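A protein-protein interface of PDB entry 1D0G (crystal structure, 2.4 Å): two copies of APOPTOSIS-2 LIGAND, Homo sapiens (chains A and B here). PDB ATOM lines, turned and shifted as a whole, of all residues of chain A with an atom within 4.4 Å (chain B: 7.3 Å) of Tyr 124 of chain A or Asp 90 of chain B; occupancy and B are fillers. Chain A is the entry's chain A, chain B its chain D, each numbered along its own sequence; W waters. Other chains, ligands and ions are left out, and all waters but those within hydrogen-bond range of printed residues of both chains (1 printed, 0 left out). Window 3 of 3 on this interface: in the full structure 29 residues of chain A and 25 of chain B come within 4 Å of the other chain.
Water W1 lies within hydrogen-bond range of O of Tyr 124 of chain A (2.8 Å), OD1 of Asn 115 of chain B (3.1 Å) and NE1 of Trp 118 of chain B (3.4 Å).
The side-chain amide nitrogen (ND2) of Asn 115 of chain B lies close to the backbone NH (N) of Leu 126 of chain A, 2.8 Å away.
The guanidinium group of Arg 114 of chain B lies within hydrogen-bond range of the backbone carbonyl oxygen of Leu 126 of chain A, at 2.9 Å.
The side-chain hydroxyl (OH) of Tyr 124 of chain A is in hydrogen-bond range of the side-chain carboxylate (OD2) of Asp 90 of chain B, at 2.7 Å.
NE2 of Gln 92 of chain B is in hydrogen-bond range of OH of Tyr 124 of chain A, 2.9 Å away.
O of Tyr 124 of chain A lies within hydrogen-bond range of NE1 of Trp 118 of chain B (2.9 Å).
Tyr 124 of chain A touches just these residues of chain B: Asp 90 (2.7 Å), Gln 92 (2.9 Å), Asn 115 (3.9 Å) and Trp 118 (2.9 Å).
Asp 90 of chain B touches just one residue of chain A: Tyr 124.
Printed residues of chain A within 4 Å of Gln 92 of chain B: Tyr 124 and Leu 126.
Printed residues of chain B within 4 Å of Leu 126 of chain A: Gln 92 (3.9 Å), Arg 114 (2.9 Å) and Asn 115 (2.8 Å).
Gln 80 of chain A touches none of the printed residues of chain B.
Glu 81 of chain B touches none of the printed residues of chain A.
The nearest residue of chain B that does not touch Tyr 124 of chain A is Lys 91 of chain B (4.6 Å).
The nearest printed residue of chain A that does not touch Asp 90 of chain B is Glu 123 of chain A (5.7 Å).
The nearest printed residue of chain A that does not touch Asn 115 of chain B is Phe 79 of chain A (6.2 Å).
The side-chain amide nitrogen (ND2) of Asn 149 of chain B is in hydrogen-bond range of the backbone carbonyl oxygen (O) of Gln 92 of chain B, 3.0 Å away.
The guanidinium group of Arg 114 of chain B sits close to the side-chain amide nitrogen of Asn 115 of chain B.
The backbone NH of Gly 125 of chain A is in hydrogen-bond range of the backbone carbonyl oxygen of Phe 79 of chain A, at 2.8 Å.
The side-chain amide oxygen of Asn 115 of chain B lies within hydrogen-bond range of the indole nitrogen of Trp 118 of chain B (3.3 Å).
Among the printed residues, merely in contact across the chains: Ala 122 of chain A with Trp 118 of chain B (3.5 Å), Glu 123 of chain A with Trp 118 of chain B (3.6 Å), Tyr 124 of chain A with Asn 115 of chain B (3.9 Å), Gly 125 of chain A with Asn 115 of chain B (3.4 Å) and Leu 126 of chain A with Gln 92 of chain B (3.9 Å).
Of the 7 printed residues of chain A, 5 touch a printed residue of chain B.
Hydrophobic or aromatic side chains of chain A within 4 Å of the printed part of chain B: Ala 122, Tyr 124 and Leu 126.
Hydrophobic or aromatic side chains of chain B that line the printed part of chain A: Trp 118.
Among the printed residues, 10 pairs touch across the chains.
Among the printed residues, no Asp or Glu carboxylate lies within 4 Å of a Lys or Arg side-chain nitrogen of the other chain.
No position is printed for both chains.
Of the 10 pairs that touch across the chains among the printed residues, none has its exchanged pair printed and touching as well.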
ATOM      1  N   PHE A  79      -0.674 -16.874  36.176  1.00  0.00           N
ATOM      2  CA  PHE A  79       0.019 -15.836  36.927  1.00  0.00           C
ATOM      3  C   PHE A  79      -0.670 -14.468  36.926  1.00  0.00           C
ATOM      4  O   PHE A  79      -1.283 -14.046  35.920  1.00  0.00           O
ATOM      5  CB  PHE A  79       1.437 -15.672  36.410  1.00  0.00           C
ATOM      6  CG  PHE A  79       1.498 -15.223  34.988  1.00  0.00           C
ATOM      7  CD1 PHE A  79       1.308 -13.897  34.659  1.00  0.00           C
ATOM      8  CD2 PHE A  79       1.830 -16.126  33.980  1.00  0.00           C
ATOM      9  CE1 PHE A  79       1.437 -13.474  33.335  1.00  0.00           C
ATOM     10  CE2 PHE A  79       1.958 -15.722  32.662  1.00  0.00           C
ATOM     11  CZ  PHE A  79       1.777 -14.384  32.337  1.00  0.00           C
ATOM     12  N   GLN A  80      -0.531 -13.757  38.049  1.00  0.00           N
ATOM     13  CA  GLN A  80      -1.115 -12.428  38.202  1.00  0.00           C
ATOM     14  C   GLN A  80       0.077 -11.484  38.296  1.00  0.00           C
ATOM     15  O   GLN A  80       0.358 -10.935  39.345  1.00  0.00           O
ATOM     16  CB  GLN A  80      -1.970 -12.369  39.479  1.00  0.00           C
ATOM     17  CG  GLN A  80      -3.123 -11.371  39.445  1.00  0.00           C
ATOM     18  CD  GLN A  80      -4.134 -11.592  40.577  1.00  0.00           C
ATOM     19  OE1 GLN A  80      -4.402 -12.722  40.987  1.00  0.00           O
ATOM     20  NE2 GLN A  80      -4.702 -10.510  41.078  1.00  0.00           N
ATOM     21  N   ALA A 122      -0.726  -5.923  30.131  1.00  0.00           N
ATOM     22  CA  ALA A 122      -1.062  -7.251  30.664  1.00  0.00           C
ATOM     23  C   ALA A 122      -1.054  -7.286  32.187  1.00  0.00           C
ATOM     24  O   ALA A 122      -0.084  -6.907  32.817  1.00  0.00           O
ATOM     25  CB  ALA A 122      -0.107  -8.307  30.110  1.00  0.00           C
ATOM     26  N   GLU A 123      -2.122  -7.786  32.785  1.00  0.00           N
ATOM     27  CA  GLU A 123      -2.192  -7.849  34.239  1.00  0.00           C
ATOM     28  C   GLU A 123      -2.130  -9.284  34.734  1.00  0.00           C
ATOM     29  O   GLU A 123      -1.777  -9.534  35.887  1.00  0.00           O
ATOM     30  CB  GLU A 123      -3.448  -7.123  34.728  1.00  0.00           C
ATOM     31  CG  GLU A 123      -3.514  -5.720  34.136  1.00  0.00           C
ATOM     32  CD  GLU A 123      -4.664  -4.860  34.637  1.00  0.00           C
ATOM     33  OE1 GLU A 123      -5.745  -5.387  34.966  1.00  0.00           O
ATOM     34  OE2 GLU A 123      -4.479  -3.628  34.685  1.00  0.00           O
ATOM     35  N   TYR A 124      -2.505 -10.222  33.860  1.00  0.00           N
ATOM     36  CA  TYR A 124      -2.469 -11.636  34.193  1.00  0.00           C
ATOM     37  C   TYR A 124      -2.369 -12.536  32.961  1.00  0.00           C
ATOM     38  O   TYR A 124      -2.616 -12.094  31.823  1.00  0.00           O
ATOM     39  CB  TYR A 124      -3.660 -12.027  35.077  1.00  0.00           C
ATOM     40  CG  TYR A 124      -5.013 -11.814  34.447  1.00  0.00           C
ATOM     41  CD1 TYR A 124      -5.521 -12.747  33.530  1.00  0.00           C
ATOM     42  CD2 TYR A 124      -5.815 -10.694  34.788  1.00  0.00           C
ATOM     43  CE1 TYR A 124      -6.749 -12.596  32.977  1.00  0.00           C
ATOM     44  CE2 TYR A 124      -7.086 -10.532  34.231  1.00  0.00           C
ATOM     45  CZ  TYR A 124      -7.533 -11.509  33.319  1.00  0.00           C
ATOM     46  OH  TYR A 124      -8.768 -11.487  32.743  1.00  0.00           O
ATOM     47  N   GLY A 125      -2.000 -13.795  33.211  1.00  0.00           N
ATOM     48  CA  GLY A 125      -1.844 -14.784  32.166  1.00  0.00           C
ATOM     49  C   GLY A 125      -2.481 -16.123  32.517  1.00  0.00           C
ATOM     50  O   GLY A 125      -2.327 -16.625  33.633  1.00  0.00           O
ATOM     51  N   LEU A 126      -3.221 -16.673  31.558  1.00  0.00           N
ATOM     52  CA  LEU A 126      -3.925 -17.940  31.687  1.00  0.00           C
ATOM     53  C   LEU A 126      -3.500 -18.752  30.466  1.00  0.00           C
ATOM     54  O   LEU A 126      -3.943 -18.510  29.359  1.00  0.00           O
ATOM     55  CB  LEU A 126      -5.434 -17.713  31.644  1.00  0.00           C
ATOM     56  CG  LEU A 126      -6.036 -16.653  32.571  1.00  0.00           C
ATOM     57  CD1 LEU A 126      -7.522 -16.599  32.341  1.00  0.00           C
ATOM     58  CD2 LEU A 126      -5.725 -16.944  34.032  1.00  0.00           C
ATOM     59  N   GLU B  81     -13.419  -8.090  17.916  1.00  0.00           N
ATOM     60  CA  GLU B  81     -13.527  -7.052  18.943  1.00  0.00           C
ATOM     61  C   GLU B  81     -13.185  -5.579  18.665  1.00  0.00           C
ATOM     62  O   GLU B  81     -12.301  -5.257  17.868  1.00  0.00           O
ATOM     63  CB  GLU B  81     -12.681  -7.449  20.099  1.00  0.00           C
ATOM     64  CG  GLU B  81     -11.259  -7.225  19.842  1.00  0.00           C
ATOM     65  CD  GLU B  81     -10.568  -7.192  21.124  1.00  0.00           C
ATOM     66  OE1 GLU B  81     -11.214  -6.949  22.161  1.00  0.00           O
ATOM     67  OE2 GLU B  81      -9.381  -7.459  21.110  1.00  0.00           O
ATOM     68  N   THR B  87     -16.456  -0.377  30.015  1.00  0.00           N
ATOM     69  CA  THR B  87     -16.140  -1.727  30.499  1.00  0.00           C
ATOM     70  C   THR B  87     -14.687  -2.066  30.247  1.00  0.00           C
ATOM     71  O   THR B  87     -13.997  -1.395  29.476  1.00  0.00           O
ATOM     72  CB  THR B  87     -16.939  -2.849  29.778  1.00  0.00           C
ATOM     73  OG1 THR B  87     -18.248  -2.389  29.451  1.00  0.00           O
ATOM     74  CG2 THR B  87     -17.079  -4.066  30.689  1.00  0.00           C
ATOM     75  N   LYS B  88     -14.207  -3.055  30.989  1.00  0.00           N
ATOM     76  CA  LYS B  88     -12.858  -3.573  30.823  1.00  0.00           C
ATOM     77  C   LYS B  88     -12.948  -4.516  29.613  1.00  0.00           C
ATOM     78  O   LYS B  88     -14.035  -4.966  29.273  1.00  0.00           O
ATOM     79  CB  LYS B  88     -12.481  -4.321  32.095  1.00  0.00           C
ATOM     80  CG  LYS B  88     -12.729  -3.481  33.378  1.00  0.00           C
ATOM     81  CD  LYS B  88     -12.326  -4.222  34.642  1.00  0.00           C
ATOM     82  CE  LYS B  88     -11.204  -5.190  34.335  1.00  0.00           C
ATOM     83  NZ  LYS B  88     -10.874  -5.943  35.549  1.00  0.00           N
ATOM     84  N   ASN B  89     -11.831  -4.855  28.984  1.00  0.00           N
ATOM     85  CA  ASN B  89     -11.931  -5.735  27.822  1.00  0.00           C
ATOM     86  C   ASN B  89     -11.226  -7.100  27.949  1.00  0.00           C
ATOM     87  O   ASN B  89     -11.350  -7.958  27.074  1.00  0.00           O
ATOM     88  CB  ASN B  89     -11.468  -4.995  26.565  1.00  0.00           C
ATOM     89  CG  ASN B  89     -12.063  -5.575  25.299  1.00  0.00           C
ATOM     90  OD1 ASN B  89     -12.932  -6.441  25.348  1.00  0.00           O
ATOM     91  ND2 ASN B  89     -11.610  -5.097  24.159  1.00  0.00           N
ATOM     92  N   ASP B  90     -10.483  -7.294  29.033  1.00  0.00           N
ATOM     93  CA  ASP B  90      -9.785  -8.551  29.255  1.00  0.00           C
ATOM     94  C   ASP B  90     -10.795  -9.700  29.285  1.00  0.00           C
ATOM     95  O   ASP B  90     -11.849  -9.580  29.906  1.00  0.00           O
ATOM     96  CB  ASP B  90      -8.955  -8.480  30.549  1.00  0.00           C
ATOM     97  CG  ASP B  90      -9.795  -8.165  31.781  1.00  0.00           C
ATOM     98  OD1 ASP B  90     -10.585  -7.196  31.759  1.00  0.00           O
ATOM     99  OD2 ASP B  90      -9.666  -8.893  32.774  1.00  0.00           O
ATOM    100  N   LYS B  91     -10.541 -10.747  28.499  1.00  0.00           N
ATOM    101  CA  LYS B  91     -11.433 -11.917  28.440  1.00  0.00           C
ATOM    102  C   LYS B  91     -10.772 -13.188  28.955  1.00  0.00           C
ATOM    103  O   LYS B  91      -9.616 -13.439  28.684  1.00  0.00           O
ATOM    104  CB  LYS B  91     -11.882 -12.188  27.011  1.00  0.00           C
ATOM    105  CG  LYS B  91     -12.742 -11.109  26.368  1.00  0.00           C
ATOM    106  CD  LYS B  91     -12.781 -11.345  24.838  1.00  0.00           C
ATOM    107  CE  LYS B  91     -13.691 -10.365  24.093  1.00  0.00           C
ATOM    108  NZ  LYS B  91     -13.250  -8.987  24.276  1.00  0.00           N
ATOM    109  N   GLN B  92     -11.526 -13.976  29.714  1.00  0.00           N
ATOM    110  CA  GLN B  92     -11.055 -15.249  30.234  1.00  0.00           C
ATOM    111  C   GLN B  92     -11.891 -16.306  29.523  1.00  0.00           C
ATOM    112  O   GLN B  92     -13.098 -16.417  29.738  1.00  0.00           O
ATOM    113  CB  GLN B  92     -11.229 -15.331  31.751  1.00  0.00           C
ATOM    114  CG  GLN B  92     -10.543 -14.199  32.431  1.00  0.00           C
ATOM    115  CD  GLN B  92     -10.628 -14.270  33.947  1.00  0.00           C
ATOM    116  OE1 GLN B  92     -11.108 -15.272  34.521  1.00  0.00           O
ATOM    117  NE2 GLN B  92     -10.123 -13.219  34.616  1.00  0.00           N
ATOM    118  N   ARG B 114      -7.539 -19.614  28.771  1.00  0.00           N
ATOM    119  CA  ARG B 114      -6.716 -18.682  28.000  1.00  0.00           C
ATOM    120  C   ARG B 114      -7.248 -17.277  28.289  1.00  0.00           C
ATOM    121  O   ARG B 114      -8.440 -17.093  28.538  1.00  0.00           O
ATOM    122  CB  ARG B 114      -6.805 -18.993  26.493  1.00  0.00           C
ATOM    123  CG  ARG B 114      -5.991 -20.220  26.036  1.00  0.00           C
ATOM    124  CD  ARG B 114      -4.520 -19.894  25.762  1.00  0.00           C
ATOM    125  NE  ARG B 114      -4.111 -18.685  26.468  1.00  0.00           N
ATOM    126  CZ  ARG B 114      -3.586 -17.611  25.895  1.00  0.00           C
ATOM    127  NH1 ARG B 114      -3.361 -17.579  24.580  1.00  0.00           N
ATOM    128  NH2 ARG B 114      -3.405 -16.522  26.630  1.00  0.00           N
ATOM    129  N   ASN B 115      -6.363 -16.294  28.230  1.00  0.00           N
ATOM    130  CA  ASN B 115      -6.746 -14.902  28.396  1.00  0.00           C
ATOM    131  C   ASN B 115      -6.547 -14.276  27.017  1.00  0.00           C
ATOM    132  O   ASN B 115      -5.682 -14.707  26.265  1.00  0.00           O
ATOM    133  CB  ASN B 115      -5.852 -14.215  29.433  1.00  0.00           C
ATOM    134  CG  ASN B 115      -4.419 -14.046  28.969  1.00  0.00           C
ATOM    135  OD1 ASN B 115      -4.069 -13.041  28.359  1.00  0.00           O
ATOM    136  ND2 ASN B 115      -3.583 -15.000  29.288  1.00  0.00           N
ATOM    137  N   SER B 116      -7.359 -13.292  26.663  1.00  0.00           N
ATOM    138  CA  SER B 116      -7.212 -12.645  25.362  1.00  0.00           C
ATOM    139  C   SER B 116      -5.993 -11.732  25.357  1.00  0.00           C
ATOM    140  O   SER B 116      -5.547 -11.303  26.415  1.00  0.00           O
ATOM    141  CB  SER B 116      -8.430 -11.785  25.087  1.00  0.00           C
ATOM    142  OG  SER B 116      -8.580 -10.838  26.140  1.00  0.00           O
ATOM    143  N   CYS B 117      -5.461 -11.433  24.168  1.00  0.00           N
ATOM    144  CA  CYS B 117      -4.339 -10.520  24.029  1.00  0.00           C
ATOM    145  C   CYS B 117      -4.744  -9.175  24.717  1.00  0.00           C
ATOM    146  O   CYS B 117      -5.882  -8.691  24.566  1.00  0.00           O
ATOM    147  CB  CYS B 117      -4.074 -10.281  22.561  1.00  0.00           C
ATOM    148  SG  CYS B 117      -2.735  -9.127  22.237  1.00  0.00           S
ATOM    149  N   TRP B 118      -3.804  -8.589  25.459  1.00  0.00           N
ATOM    150  CA  TRP B 118      -4.078  -7.364  26.190  1.00  0.00           C
ATOM    151  C   TRP B 118      -3.863  -6.086  25.382  1.00  0.00           C
ATOM    152  O   TRP B 118      -4.401  -5.053  25.731  1.00  0.00           O
ATOM    153  CB  TRP B 118      -3.255  -7.305  27.483  1.00  0.00           C
ATOM    154  CG  TRP B 118      -3.607  -8.325  28.545  1.00  0.00           C
ATOM    155  CD1 TRP B 118      -3.079  -9.580  28.691  1.00  0.00           C
ATOM    156  CD2 TRP B 118      -4.463  -8.117  29.674  1.00  0.00           C
ATOM    157  NE1 TRP B 118      -3.542 -10.158  29.849  1.00  0.00           N
ATOM    158  CE2 TRP B 118      -4.396  -9.285  30.472  1.00  0.00           C
ATOM    159  CE3 TRP B 118      -5.279  -7.057  30.090  1.00  0.00           C
ATOM    160  CZ2 TRP B 118      -5.123  -9.424  31.667  1.00  0.00           C
ATOM    161  CZ3 TRP B 118      -6.005  -7.193  31.273  1.00  0.00           C
ATOM    162  CH2 TRP B 118      -5.920  -8.372  32.051  1.00  0.00           C
ATOM    163  N   ASN B 149     -18.050 -16.964  28.323  1.00  0.00           N
ATOM    164  CA  ASN B 149     -18.218 -16.244  27.054  1.00  0.00           C
ATOM    165  C   ASN B 149     -18.846 -17.062  25.917  1.00  0.00           C
ATOM    166  O   ASN B 149     -18.319 -17.081  24.791  1.00  0.00           O
ATOM    167  CB  ASN B 149     -16.862 -15.668  26.592  1.00  0.00           C
ATOM    168  CG  ASN B 149     -16.319 -14.597  27.541  1.00  0.00           C
ATOM    169  OD1 ASN B 149     -16.946 -13.556  27.741  1.00  0.00           O
ATOM    170  ND2 ASN B 149     -15.160 -14.863  28.148  1.00  0.00           N
HETATM  171  O   HOH W   1      -1.198 -12.534  29.462  1.00  0.00           O
